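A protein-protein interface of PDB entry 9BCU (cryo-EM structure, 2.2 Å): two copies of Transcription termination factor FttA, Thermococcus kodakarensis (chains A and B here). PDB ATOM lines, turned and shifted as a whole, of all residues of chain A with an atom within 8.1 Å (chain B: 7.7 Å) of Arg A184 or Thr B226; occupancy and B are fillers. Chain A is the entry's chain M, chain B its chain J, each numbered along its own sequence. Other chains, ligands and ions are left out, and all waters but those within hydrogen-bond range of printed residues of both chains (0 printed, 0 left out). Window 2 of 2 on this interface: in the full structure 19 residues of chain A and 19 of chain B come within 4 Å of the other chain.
The indole nitrogen of Trp A185 lies within hydrogen-bond range of the side-chain carboxylate of Asp B233 (3.2 Å).
O of Leu B642 is in hydrogen-bond range of NE of Arg A187 (3.0 Å).
The side-chain carboxylate of Glu B196 is in hydrogen-bond range of the side-chain amide nitrogen of Asn B641.
The backbone carbonyl oxygen (O) of Thr B226 is in hydrogen-bond range of the guanidinium group (NH1) of Arg B199 (3.4 Å).
The side-chain hydroxyl (OG1) of Thr B226 is in hydrogen-bond range of the side-chain carboxylate (OD2) of Asp B224.
A ring nitrogen (ND1) of His B231 sits close to the side-chain carboxylate of Asp B233 (3.4 Å).
The backbone NH (N) of Arg A184 is in hydrogen-bond range of the side-chain carboxylate (OD1) of Asp A207 (3.5 Å).
The guanidinium group (NE) of Arg A646 sits at hydrogen-bond distance from the backbone carbonyl oxygen (O) of Lys A648 (3.1 Å).
Among the printed residues, merely in contact across the chains: Arg A184 with Thr B226 (3.9 Å), Trp A185 with Leu B642 (3.6 Å) and Arg A646 with Asn B641 (3.3 Å).
Arg A184 touches just one residue of chain B: Thr B226 (3.9 Å).
Printed residues of chain A within 4 Å of Asn B641: Arg A646 (3.3 Å).
Printed residues of chain A within 4 Å of Leu B642: Trp A185 (3.6 Å) and Arg A187 (3.0 Å).
Lys B227 touches none of the printed residues of chain A.
Asp A207 touches none of the printed residues of chain B.
The nearest printed residue of chain A that does not touch Thr B226 is Arg A646 (8.2 Å).
The nearest printed residue of chain B that does not touch Arg A187 is Asn B641 (6.2 Å).
Printed residues of chain A that touch a printed residue of chain B: Arg A184, Trp A185, Arg A187 and Arg A646.
Hydrophobic or aromatic side chains of chain A that line the printed part of chain B: Trp A185.
Of the 17 printed residues of chain B, 4 touch a printed residue of chain A.
Among the printed residues, 5 pairs touch across the chains.
No position is printed for both chains.
Of the 5 pairs that touch across the chains among the printed residues, none has its exchanged pair printed and touching as well.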
ATOM      1  N   TYR A 181     -21.248  24.066 -25.567  1.00  0.00           N
ATOM      2  CA  TYR A 181     -20.568  22.972 -24.891  1.00  0.00           C
ATOM      3  C   TYR A 181     -19.880  23.479 -23.632  1.00  0.00           C
ATOM      4  O   TYR A 181     -19.267  24.551 -23.636  1.00  0.00           O
ATOM      5  CB  TYR A 181     -19.542  22.316 -25.820  1.00  0.00           C
ATOM      6  CG  TYR A 181     -18.744  21.206 -25.179  1.00  0.00           C
ATOM      7  CD1 TYR A 181     -19.338  19.992 -24.864  1.00  0.00           C
ATOM      8  CD2 TYR A 181     -17.396  21.370 -24.892  1.00  0.00           C
ATOM      9  CE1 TYR A 181     -18.613  18.972 -24.279  1.00  0.00           C
ATOM     10  CE2 TYR A 181     -16.662  20.357 -24.307  1.00  0.00           C
ATOM     11  CZ  TYR A 181     -17.275  19.161 -24.002  1.00  0.00           C
ATOM     12  OH  TYR A 181     -16.550  18.148 -23.420  1.00  0.00           O
ATOM     13  N   LYS A 182     -19.989  22.706 -22.556  1.00  0.00           N
ATOM     14  CA  LYS A 182     -19.342  23.022 -21.290  1.00  0.00           C
ATOM     15  C   LYS A 182     -18.034  22.247 -21.200  1.00  0.00           C
ATOM     16  O   LYS A 182     -18.035  21.012 -21.260  1.00  0.00           O
ATOM     17  CB  LYS A 182     -20.254  22.683 -20.110  1.00  0.00           C
ATOM     18  CG  LYS A 182     -21.563  23.454 -20.099  1.00  0.00           C
ATOM     19  CD  LYS A 182     -21.619  24.426 -18.933  1.00  0.00           C
ATOM     20  CE  LYS A 182     -23.043  24.879 -18.662  1.00  0.00           C
ATOM     21  NZ  LYS A 182     -23.835  24.991 -19.917  1.00  0.00           N
ATOM     22  N   SER A 183     -16.928  22.970 -21.060  1.00  0.00           N
ATOM     23  CA  SER A 183     -15.620  22.337 -21.000  1.00  0.00           C
ATOM     24  C   SER A 183     -15.440  21.588 -19.684  1.00  0.00           C
ATOM     25  O   SER A 183     -15.949  21.991 -18.635  1.00  0.00           O
ATOM     26  CB  SER A 183     -14.515  23.380 -21.164  1.00  0.00           C
ATOM     27  OG  SER A 183     -14.967  24.480 -21.933  1.00  0.00           O
ATOM     28  N   ARG A 184     -14.705  20.477 -19.751  1.00  0.00           N
ATOM     29  CA  ARG A 184     -14.437  19.693 -18.551  1.00  0.00           C
ATOM     30  C   ARG A 184     -13.267  20.263 -17.759  1.00  0.00           C
ATOM     31  O   ARG A 184     -13.277  20.232 -16.523  1.00  0.00           O
ATOM     32  CB  ARG A 184     -14.170  18.232 -18.919  1.00  0.00           C
ATOM     33  CG  ARG A 184     -15.081  17.666 -20.000  1.00  0.00           C
ATOM     34  CD  ARG A 184     -16.560  17.824 -19.636  1.00  0.00           C
ATOM     35  NE  ARG A 184     -17.048  16.824 -18.688  1.00  0.00           N
ATOM     36  CZ  ARG A 184     -17.050  15.509 -18.879  1.00  0.00           C
ATOM     37  NH1 ARG A 184     -16.673  14.970 -20.029  1.00  0.00           N
ATOM     38  NH2 ARG A 184     -17.466  14.714 -17.898  1.00  0.00           N
ATOM     39  N   TRP A 185     -12.254  20.783 -18.447  1.00  0.00           N
ATOM     40  CA  TRP A 185     -11.092  21.355 -17.784  1.00  0.00           C
ATOM     41  C   TRP A 185     -10.529  22.478 -18.640  1.00  0.00           C
ATOM     42  O   TRP A 185     -10.659  22.470 -19.868  1.00  0.00           O
ATOM     43  CB  TRP A 185     -10.015  20.297 -17.522  1.00  0.00           C
ATOM     44  CG  TRP A 185      -9.767  19.388 -18.686  1.00  0.00           C
ATOM     45  CD1 TRP A 185     -10.354  18.179 -18.920  1.00  0.00           C
ATOM     46  CD2 TRP A 185      -8.865  19.614 -19.776  1.00  0.00           C
ATOM     47  NE1 TRP A 185      -9.874  17.639 -20.089  1.00  0.00           N
ATOM     48  CE2 TRP A 185      -8.958  18.500 -20.633  1.00  0.00           C
ATOM     49  CE3 TRP A 185      -7.987  20.650 -20.110  1.00  0.00           C
ATOM     50  CZ2 TRP A 185      -8.208  18.392 -21.802  1.00  0.00           C
ATOM     51  CZ3 TRP A 185      -7.244  20.541 -21.271  1.00  0.00           C
ATOM     52  CH2 TRP A 185      -7.358  19.421 -22.102  1.00  0.00           C
ATOM     53  N   ILE A 186      -9.905  23.450 -17.977  1.00  0.00           N
ATOM     54  CA  ILE A 186      -9.260  24.579 -18.637  1.00  0.00           C
ATOM     55  C   ILE A 186      -7.847  24.707 -18.089  1.00  0.00           C
ATOM     56  O   ILE A 186      -7.651  24.737 -16.869  1.00  0.00           O
ATOM     57  CB  ILE A 186     -10.039  25.892 -18.426  1.00  0.00           C
ATOM     58  CG1 ILE A 186     -11.455  25.778 -18.989  1.00  0.00           C
ATOM     59  CG2 ILE A 186      -9.304  27.059 -19.066  1.00  0.00           C
ATOM     60  CD1 ILE A 186     -12.484  26.524 -18.181  1.00  0.00           C
ATOM     61  N   ARG A 187      -6.866  24.779 -18.986  1.00  0.00           N
ATOM     62  CA  ARG A 187      -5.481  24.996 -18.599  1.00  0.00           C
ATOM     63  C   ARG A 187      -4.847  25.998 -19.551  1.00  0.00           C
ATOM     64  O   ARG A 187      -5.271  26.139 -20.702  1.00  0.00           O
ATOM     65  CB  ARG A 187      -4.683  23.682 -18.582  1.00  0.00           C
ATOM     66  CG  ARG A 187      -4.204  23.213 -19.944  1.00  0.00           C
ATOM     67  CD  ARG A 187      -4.041  21.704 -19.981  1.00  0.00           C
ATOM     68  NE  ARG A 187      -2.811  21.270 -19.330  1.00  0.00           N
ATOM     69  CZ  ARG A 187      -1.802  20.679 -19.955  1.00  0.00           C
ATOM     70  NH1 ARG A 187      -1.838  20.442 -21.256  1.00  0.00           N
ATOM     71  NH2 ARG A 187      -0.730  20.316 -19.257  1.00  0.00           N
ATOM     72  N   THR A 206      -8.548  23.838 -23.807  1.00  0.00           N
ATOM     73  CA  THR A 206      -9.695  23.167 -23.218  1.00  0.00           C
ATOM     74  C   THR A 206      -9.765  21.744 -23.762  1.00  0.00           C
ATOM     75  O   THR A 206      -8.908  21.308 -24.536  1.00  0.00           O
ATOM     76  CB  THR A 206     -10.993  23.928 -23.506  1.00  0.00           C
ATOM     77  OG1 THR A 206     -11.155  24.080 -24.921  1.00  0.00           O
ATOM     78  CG2 THR A 206     -10.962  25.302 -22.854  1.00  0.00           C
ATOM     79  N   ASP A 207     -10.799  21.014 -23.353  1.00  0.00           N
ATOM     80  CA  ASP A 207     -10.992  19.658 -23.849  1.00  0.00           C
ATOM     81  C   ASP A 207     -11.521  19.621 -25.277  1.00  0.00           C
ATOM     82  O   ASP A 207     -11.519  18.550 -25.892  1.00  0.00           O
ATOM     83  CB  ASP A 207     -11.943  18.889 -22.929  1.00  0.00           C
ATOM     84  CG  ASP A 207     -13.369  19.388 -23.016  1.00  0.00           C
ATOM     85  OD1 ASP A 207     -13.571  20.621 -23.007  1.00  0.00           O
ATOM     86  OD2 ASP A 207     -14.290  18.549 -23.095  1.00  0.00           O
ATOM     87  N   GLU A 208     -11.967  20.752 -25.815  1.00  0.00           N
ATOM     88  CA  GLU A 208     -12.520  20.816 -27.163  1.00  0.00           C
ATOM     89  C   GLU A 208     -11.771  21.766 -28.083  1.00  0.00           C
ATOM     90  O   GLU A 208     -11.518  21.422 -29.239  1.00  0.00           O
ATOM     91  CB  GLU A 208     -14.000  21.225 -27.100  1.00  0.00           C
ATOM     92  CG  GLU A 208     -14.635  21.500 -28.453  1.00  0.00           C
ATOM     93  CD  GLU A 208     -15.161  20.243 -29.119  1.00  0.00           C
ATOM     94  OE1 GLU A 208     -15.041  19.154 -28.520  1.00  0.00           O
ATOM     95  OE2 GLU A 208     -15.694  20.345 -30.244  1.00  0.00           O
ATOM     96  N   ASP A 331     -16.956  26.534 -27.253  1.00  0.00           N
ATOM     97  CA  ASP A 331     -17.087  26.791 -25.828  1.00  0.00           C
ATOM     98  C   ASP A 331     -16.456  28.101 -25.372  1.00  0.00           C
ATOM     99  O   ASP A 331     -16.593  28.449 -24.195  1.00  0.00           O
ATOM    100  CB  ASP A 331     -16.475  25.636 -25.018  1.00  0.00           C
ATOM    101  CG  ASP A 331     -15.079  25.276 -25.481  1.00  0.00           C
ATOM    102  OD1 ASP A 331     -14.681  25.722 -26.577  1.00  0.00           O
ATOM    103  OD2 ASP A 331     -14.377  24.548 -24.749  1.00  0.00           O
ATOM    104  N   ILE A 352     -15.212  31.165 -21.280  1.00  0.00           N
ATOM    105  CA  ILE A 352     -15.191  29.741 -21.596  1.00  0.00           C
ATOM    106  C   ILE A 352     -16.407  29.082 -20.959  1.00  0.00           C
ATOM    107  O   ILE A 352     -16.619  29.187 -19.746  1.00  0.00           O
ATOM    108  CB  ILE A 352     -13.890  29.084 -21.118  1.00  0.00           C
ATOM    109  CG1 ILE A 352     -12.685  29.769 -21.764  1.00  0.00           C
ATOM    110  CG2 ILE A 352     -13.893  27.601 -21.445  1.00  0.00           C
ATOM    111  CD1 ILE A 352     -11.375  29.462 -21.085  1.00  0.00           C
ATOM    112  N   LEU A 356     -18.769  29.005 -16.856  1.00  0.00           N
ATOM    113  CA  LEU A 356     -17.864  28.091 -16.168  1.00  0.00           C
ATOM    114  C   LEU A 356     -16.615  28.815 -15.677  1.00  0.00           C
ATOM    115  O   LEU A 356     -16.200  28.643 -14.525  1.00  0.00           O
ATOM    116  CB  LEU A 356     -17.492  26.933 -17.094  1.00  0.00           C
ATOM    117  CG  LEU A 356     -16.590  25.847 -16.509  1.00  0.00           C
ATOM    118  CD1 LEU A 356     -17.404  24.869 -15.680  1.00  0.00           C
ATOM    119  CD2 LEU A 356     -15.849  25.123 -17.617  1.00  0.00           C
ATOM    120  N   ARG A 646      -3.914  24.557 -14.268  1.00  0.00           N
ATOM    121  CA  ARG A 646      -5.301  24.139 -14.423  1.00  0.00           C
ATOM    122  C   ARG A 646      -6.200  25.083 -13.636  1.00  0.00           C
ATOM    123  O   ARG A 646      -6.030  25.244 -12.423  1.00  0.00           O
ATOM    124  CB  ARG A 646      -5.482  22.698 -13.952  1.00  0.00           C
ATOM    125  CG  ARG A 646      -6.692  21.999 -14.546  1.00  0.00           C
ATOM    126  CD  ARG A 646      -7.345  21.077 -13.532  1.00  0.00           C
ATOM    127  NE  ARG A 646      -8.605  20.528 -14.020  1.00  0.00           N
ATOM    128  CZ  ARG A 646      -8.931  19.244 -13.971  1.00  0.00           C
ATOM    129  NH1 ARG A 646      -8.107  18.341 -13.464  1.00  0.00           N
ATOM    130  NH2 ARG A 646     -10.113  18.856 -14.440  1.00  0.00           N
ATOM    131  N   LEU A 647      -7.155  25.706 -14.325  1.00  0.00           N
ATOM    132  CA  LEU A 647      -8.060  26.669 -13.710  1.00  0.00           C
ATOM    133  C   LEU A 647      -9.396  26.051 -13.318  1.00  0.00           C
ATOM    134  O   LEU A 647      -9.879  26.273 -12.205  1.00  0.00           O
ATOM    135  CB  LEU A 647      -8.283  27.853 -14.658  1.00  0.00           C
ATOM    136  CG  LEU A 647      -7.013  28.426 -15.289  1.00  0.00           C
ATOM    137  CD1 LEU A 647      -7.352  29.299 -16.482  1.00  0.00           C
ATOM    138  CD2 LEU A 647      -6.209  29.207 -14.260  1.00  0.00           C
ATOM    139  N   LYS A 648     -10.004  25.279 -14.213  1.00  0.00           N
ATOM    140  CA  LYS A 648     -11.280  24.636 -13.925  1.00  0.00           C
ATOM    141  C   LYS A 648     -11.468  23.386 -14.777  1.00  0.00           C
ATOM    142  O   LYS A 648     -11.110  22.283 -14.364  1.00  0.00           O
ATOM    143  CB  LYS A 648     -12.437  25.611 -14.157  1.00  0.00           C
ATOM    144  CG  LYS A 648     -13.812  24.975 -14.061  1.00  0.00           C
ATOM    145  CD  LYS A 648     -14.752  25.823 -13.221  1.00  0.00           C
ATOM    146  CE  LYS A 648     -14.506  25.615 -11.736  1.00  0.00           C
ATOM    147  NZ  LYS A 648     -15.434  26.426 -10.902  1.00  0.00           N
ATOM    148  N   LEU B 191      -0.908  13.236 -15.130  1.00  0.00           N
ATOM    149  CA  LEU B 191      -2.124  12.790 -15.796  1.00  0.00           C
ATOM    150  C   LEU B 191      -3.111  12.135 -14.840  1.00  0.00           C
ATOM    151  O   LEU B 191      -4.260  11.897 -15.228  1.00  0.00           O
ATOM    152  CB  LEU B 191      -1.779  11.816 -16.925  1.00  0.00           C
ATOM    153  CG  LEU B 191      -0.500  12.120 -17.707  1.00  0.00           C
ATOM    154  CD1 LEU B 191      -0.067  10.911 -18.520  1.00  0.00           C
ATOM    155  CD2 LEU B 191      -0.696  13.331 -18.604  1.00  0.00           C
ATOM    156  N   GLU B 196      -5.784  13.446  -5.530  1.00  0.00           N
ATOM    157  CA  GLU B 196      -6.766  12.371  -5.542  1.00  0.00           C
ATOM    158  C   GLU B 196      -6.047  11.069  -5.219  1.00  0.00           C
ATOM    159  O   GLU B 196      -4.818  10.988  -5.258  1.00  0.00           O
ATOM    160  CB  GLU B 196      -7.488  12.284  -6.891  1.00  0.00           C
ATOM    161  CG  GLU B 196      -6.691  11.582  -7.976  1.00  0.00           C
ATOM    162  CD  GLU B 196      -7.419  11.550  -9.305  1.00  0.00           C
ATOM    163  OE1 GLU B 196      -8.531  10.984  -9.361  1.00  0.00           O
ATOM    164  OE2 GLU B 196      -6.881  12.092 -10.292  1.00  0.00           O
ATOM    165  N   ARG B 199      -5.637   5.892  -9.704  1.00  0.00           N
ATOM    166  CA  ARG B 199      -5.339   6.195 -11.113  1.00  0.00           C
ATOM    167  C   ARG B 199      -4.142   7.135 -11.263  1.00  0.00           C
ATOM    168  O   ARG B 199      -4.173   8.125 -11.997  1.00  0.00           O
ATOM    169  CB  ARG B 199      -6.578   6.734 -11.848  1.00  0.00           C
ATOM    170  CG  ARG B 199      -7.202   8.025 -11.326  1.00  0.00           C
ATOM    171  CD  ARG B 199      -7.459   9.001 -12.462  1.00  0.00           C
ATOM    172  NE  ARG B 199      -8.322  10.102 -12.053  1.00  0.00           N
ATOM    173  CZ  ARG B 199      -8.831  11.001 -12.884  1.00  0.00           C
ATOM    174  NH1 ARG B 199      -8.586  10.959 -14.183  1.00  0.00           N
ATOM    175  NH2 ARG B 199      -9.605  11.968 -12.398  1.00  0.00           N
ATOM    176  N   ALA B 221     -13.891   4.647  -8.473  1.00  0.00           N
ATOM    177  CA  ALA B 221     -14.715   5.352  -9.453  1.00  0.00           C
ATOM    178  C   ALA B 221     -14.769   4.615 -10.784  1.00  0.00           C
ATOM    179  O   ALA B 221     -14.775   5.241 -11.847  1.00  0.00           O
ATOM    180  CB  ALA B 221     -14.203   6.775  -9.648  1.00  0.00           C
ATOM    181  N   LEU B 222     -14.813   3.280 -10.752  1.00  0.00           N
ATOM    182  CA  LEU B 222     -14.810   2.494 -11.981  1.00  0.00           C
ATOM    183  C   LEU B 222     -16.079   2.682 -12.804  1.00  0.00           C
ATOM    184  O   LEU B 222     -16.062   2.415 -14.010  1.00  0.00           O
ATOM    185  CB  LEU B 222     -14.620   1.012 -11.657  1.00  0.00           C
ATOM    186  CG  LEU B 222     -13.288   0.392 -12.084  1.00  0.00           C
ATOM    187  CD1 LEU B 222     -13.179  -1.041 -11.588  1.00  0.00           C
ATOM    188  CD2 LEU B 222     -13.127   0.454 -13.595  1.00  0.00           C
ATOM    189  N   LYS B 223     -17.174   3.126 -12.184  1.00  0.00           N
ATOM    190  CA  LYS B 223     -18.402   3.359 -12.937  1.00  0.00           C
ATOM    191  C   LYS B 223     -18.281   4.567 -13.855  1.00  0.00           C
ATOM    192  O   LYS B 223     -18.870   4.579 -14.943  1.00  0.00           O
ATOM    193  CB  LYS B 223     -19.581   3.534 -11.980  1.00  0.00           C
ATOM    194  CG  LYS B 223     -19.872   2.312 -11.126  1.00  0.00           C
ATOM    195  CD  LYS B 223     -21.146   1.614 -11.577  1.00  0.00           C
ATOM    196  CE  LYS B 223     -21.109   0.131 -11.248  1.00  0.00           C
ATOM    197  NZ  LYS B 223     -19.937  -0.547 -11.870  1.00  0.00           N
ATOM    198  N   ASP B 224     -17.529   5.589 -13.442  1.00  0.00           N
ATOM    199  CA  ASP B 224     -17.349   6.786 -14.248  1.00  0.00           C
ATOM    200  C   ASP B 224     -16.041   6.690 -15.014  1.00  0.00           C
ATOM    201  O   ASP B 224     -14.969   6.668 -14.387  1.00  0.00           O
ATOM    202  CB  ASP B 224     -17.353   8.030 -13.369  1.00  0.00           C
ATOM    203  CG  ASP B 224     -17.444   9.312 -14.172  1.00  0.00           C
ATOM    204  OD1 ASP B 224     -17.898   9.256 -15.334  1.00  0.00           O
ATOM    205  OD2 ASP B 224     -17.061  10.376 -13.642  1.00  0.00           O
ATOM    206  N   PRO B 225     -16.069   6.621 -16.349  1.00  0.00           N
ATOM    207  CA  PRO B 225     -14.809   6.544 -17.108  1.00  0.00           C
ATOM    208  C   PRO B 225     -13.946   7.791 -16.998  1.00  0.00           C
ATOM    209  O   PRO B 225     -12.740   7.707 -17.256  1.00  0.00           O
ATOM    210  CB  PRO B 225     -15.281   6.320 -18.551  1.00  0.00           C
ATOM    211  CG  PRO B 225     -16.670   6.863 -18.584  1.00  0.00           C
ATOM    212  CD  PRO B 225     -17.251   6.599 -17.227  1.00  0.00           C
ATOM    213  N   THR B 226     -14.519   8.939 -16.629  1.00  0.00           N
ATOM    214  CA  THR B 226     -13.733  10.163 -16.531  1.00  0.00           C
ATOM    215  C   THR B 226     -12.828  10.179 -15.305  1.00  0.00           C
ATOM    216  O   THR B 226     -11.854  10.938 -15.280  1.00  0.00           O
ATOM    217  CB  THR B 226     -14.655  11.382 -16.504  1.00  0.00           C
ATOM    218  OG1 THR B 226     -15.347  11.434 -15.251  1.00  0.00           O
ATOM    219  CG2 THR B 226     -15.668  11.307 -17.635  1.00  0.00           C
ATOM    220  N   LYS B 227     -13.125   9.363 -14.291  1.00  0.00           N
ATOM    221  CA  LYS B 227     -12.321   9.309 -13.080  1.00  0.00           C
ATOM    222  C   LYS B 227     -11.630   7.974 -12.852  1.00  0.00           C
ATOM    223  O   LYS B 227     -10.713   7.911 -12.026  1.00  0.00           O
ATOM    224  CB  LYS B 227     -13.184   9.629 -11.848  1.00  0.00           C
ATOM    225  CG  LYS B 227     -13.949  10.937 -11.946  1.00  0.00           C
ATOM    226  CD  LYS B 227     -14.723  11.218 -10.669  1.00  0.00           C
ATOM    227  CE  LYS B 227     -15.969  12.042 -10.948  1.00  0.00           C
ATOM    228  NZ  LYS B 227     -16.736  12.329  -9.704  1.00  0.00           N
ATOM    229  N   ALA B 228     -12.036   6.912 -13.550  1.00  0.00           N
ATOM    230  CA  ALA B 228     -11.436   5.601 -13.336  1.00  0.00           C
ATOM    231  C   ALA B 228     -10.051   5.488 -13.958  1.00  0.00           C
ATOM    232  O   ALA B 228      -9.213   4.732 -13.455  1.00  0.00           O
ATOM    233  CB  ALA B 228     -12.344   4.508 -13.899  1.00  0.00           C
ATOM    234  N   TYR B 229      -9.792   6.220 -15.033  1.00  0.00           N
ATOM    235  CA  TYR B 229      -8.579   6.087 -15.819  1.00  0.00           C
ATOM    236  C   TYR B 229      -7.829   7.412 -15.869  1.00  0.00           C
ATOM    237  O   TYR B 229      -8.425   8.480 -15.688  1.00  0.00           O
ATOM    238  CB  TYR B 229      -8.915   5.620 -17.243  1.00  0.00           C
ATOM    239  CG  TYR B 229     -10.050   4.623 -17.299  1.00  0.00           C
ATOM    240  CD1 TYR B 229      -9.925   3.367 -16.721  1.00  0.00           C
ATOM    241  CD2 TYR B 229     -11.248   4.942 -17.923  1.00  0.00           C
ATOM    242  CE1 TYR B 229     -10.960   2.454 -16.768  1.00  0.00           C
ATOM    243  CE2 TYR B 229     -12.290   4.034 -17.974  1.00  0.00           C
ATOM    244  CZ  TYR B 229     -12.140   2.792 -17.395  1.00  0.00           C
ATOM    245  OH  TYR B 229     -13.173   1.885 -17.443  1.00  0.00           O
ATOM    246  N   PRO B 230      -6.514   7.379 -16.096  1.00  0.00           N
ATOM    247  CA  PRO B 230      -5.755   8.630 -16.209  1.00  0.00           C
ATOM    248  C   PRO B 230      -6.188   9.442 -17.421  1.00  0.00           C
ATOM    249  O   PRO B 230      -6.839   8.945 -18.343  1.00  0.00           O
ATOM    250  CB  PRO B 230      -4.303   8.156 -16.349  1.00  0.00           C
ATOM    251  CG  PRO B 230      -4.291   6.790 -15.767  1.00  0.00           C
ATOM    252  CD  PRO B 230      -5.629   6.202 -16.088  1.00  0.00           C
ATOM    253  N   HIS B 231      -5.812  10.717 -17.405  1.00  0.00           N
ATOM    254  CA  HIS B 231      -6.241  11.666 -18.429  1.00  0.00           C
ATOM    255  C   HIS B 231      -5.555  11.333 -19.747  1.00  0.00           C
ATOM    256  O   HIS B 231      -4.396  11.688 -19.969  1.00  0.00           O
ATOM    257  CB  HIS B 231      -5.928  13.092 -17.991  1.00  0.00           C
ATOM    258  CG  HIS B 231      -6.901  13.646 -16.998  1.00  0.00           C
ATOM    259  ND1 HIS B 231      -7.989  14.405 -17.367  1.00  0.00           N
ATOM    260  CD2 HIS B 231      -6.949  13.550 -15.648  1.00  0.00           C
ATOM    261  CE1 HIS B 231      -8.666  14.753 -16.287  1.00  0.00           C
ATOM    262  NE2 HIS B 231      -8.056  14.247 -15.231  1.00  0.00           N
ATOM    263  N   ASP B 233      -6.693  12.577 -22.500  1.00  0.00           N
ATOM    264  CA  ASP B 233      -6.963  13.741 -23.332  1.00  0.00           C
ATOM    265  C   ASP B 233      -5.924  14.843 -23.169  1.00  0.00           C
ATOM    266  O   ASP B 233      -6.093  15.920 -23.749  1.00  0.00           O
ATOM    267  CB  ASP B 233      -8.356  14.299 -23.021  1.00  0.00           C
ATOM    268  CG  ASP B 233      -8.689  14.242 -21.543  1.00  0.00           C
ATOM    269  OD1 ASP B 233      -7.813  13.843 -20.749  1.00  0.00           O
ATOM    270  OD2 ASP B 233      -9.830  14.596 -21.176  1.00  0.00           O
ATOM    271  N   ASN B 641      -4.731  17.810 -11.474  1.00  0.00           N
ATOM    272  CA  ASN B 641      -4.440  17.055 -12.681  1.00  0.00           C
ATOM    273  C   ASN B 641      -4.225  18.001 -13.860  1.00  0.00           C
ATOM    274  O   ASN B 641      -4.681  19.148 -13.862  1.00  0.00           O
ATOM    275  CB  ASN B 641      -5.573  16.076 -12.989  1.00  0.00           C
ATOM    276  CG  ASN B 641      -5.501  14.820 -12.144  1.00  0.00           C
ATOM    277  OD1 ASN B 641      -4.422  14.386 -11.745  1.00  0.00           O
ATOM    278  ND2 ASN B 641      -6.656  14.226 -11.869  1.00  0.00           N
ATOM    279  N   LEU B 642      -3.508  17.497 -14.869  1.00  0.00           N
ATOM    280  CA  LEU B 642      -3.173  18.254 -16.078  1.00  0.00           C
ATOM    281  C   LEU B 642      -2.418  19.540 -15.743  1.00  0.00           C
ATOM    282  O   LEU B 642      -2.610  20.579 -16.377  1.00  0.00           O
ATOM    283  CB  LEU B 642      -4.421  18.560 -16.912  1.00  0.00           C
ATOM    284  CG  LEU B 642      -5.369  17.391 -17.184  1.00  0.00           C
ATOM    285  CD1 LEU B 642      -6.804  17.882 -17.283  1.00  0.00           C
ATOM    286  CD2 LEU B 642      -4.962  16.661 -18.451  1.00  0.00           C
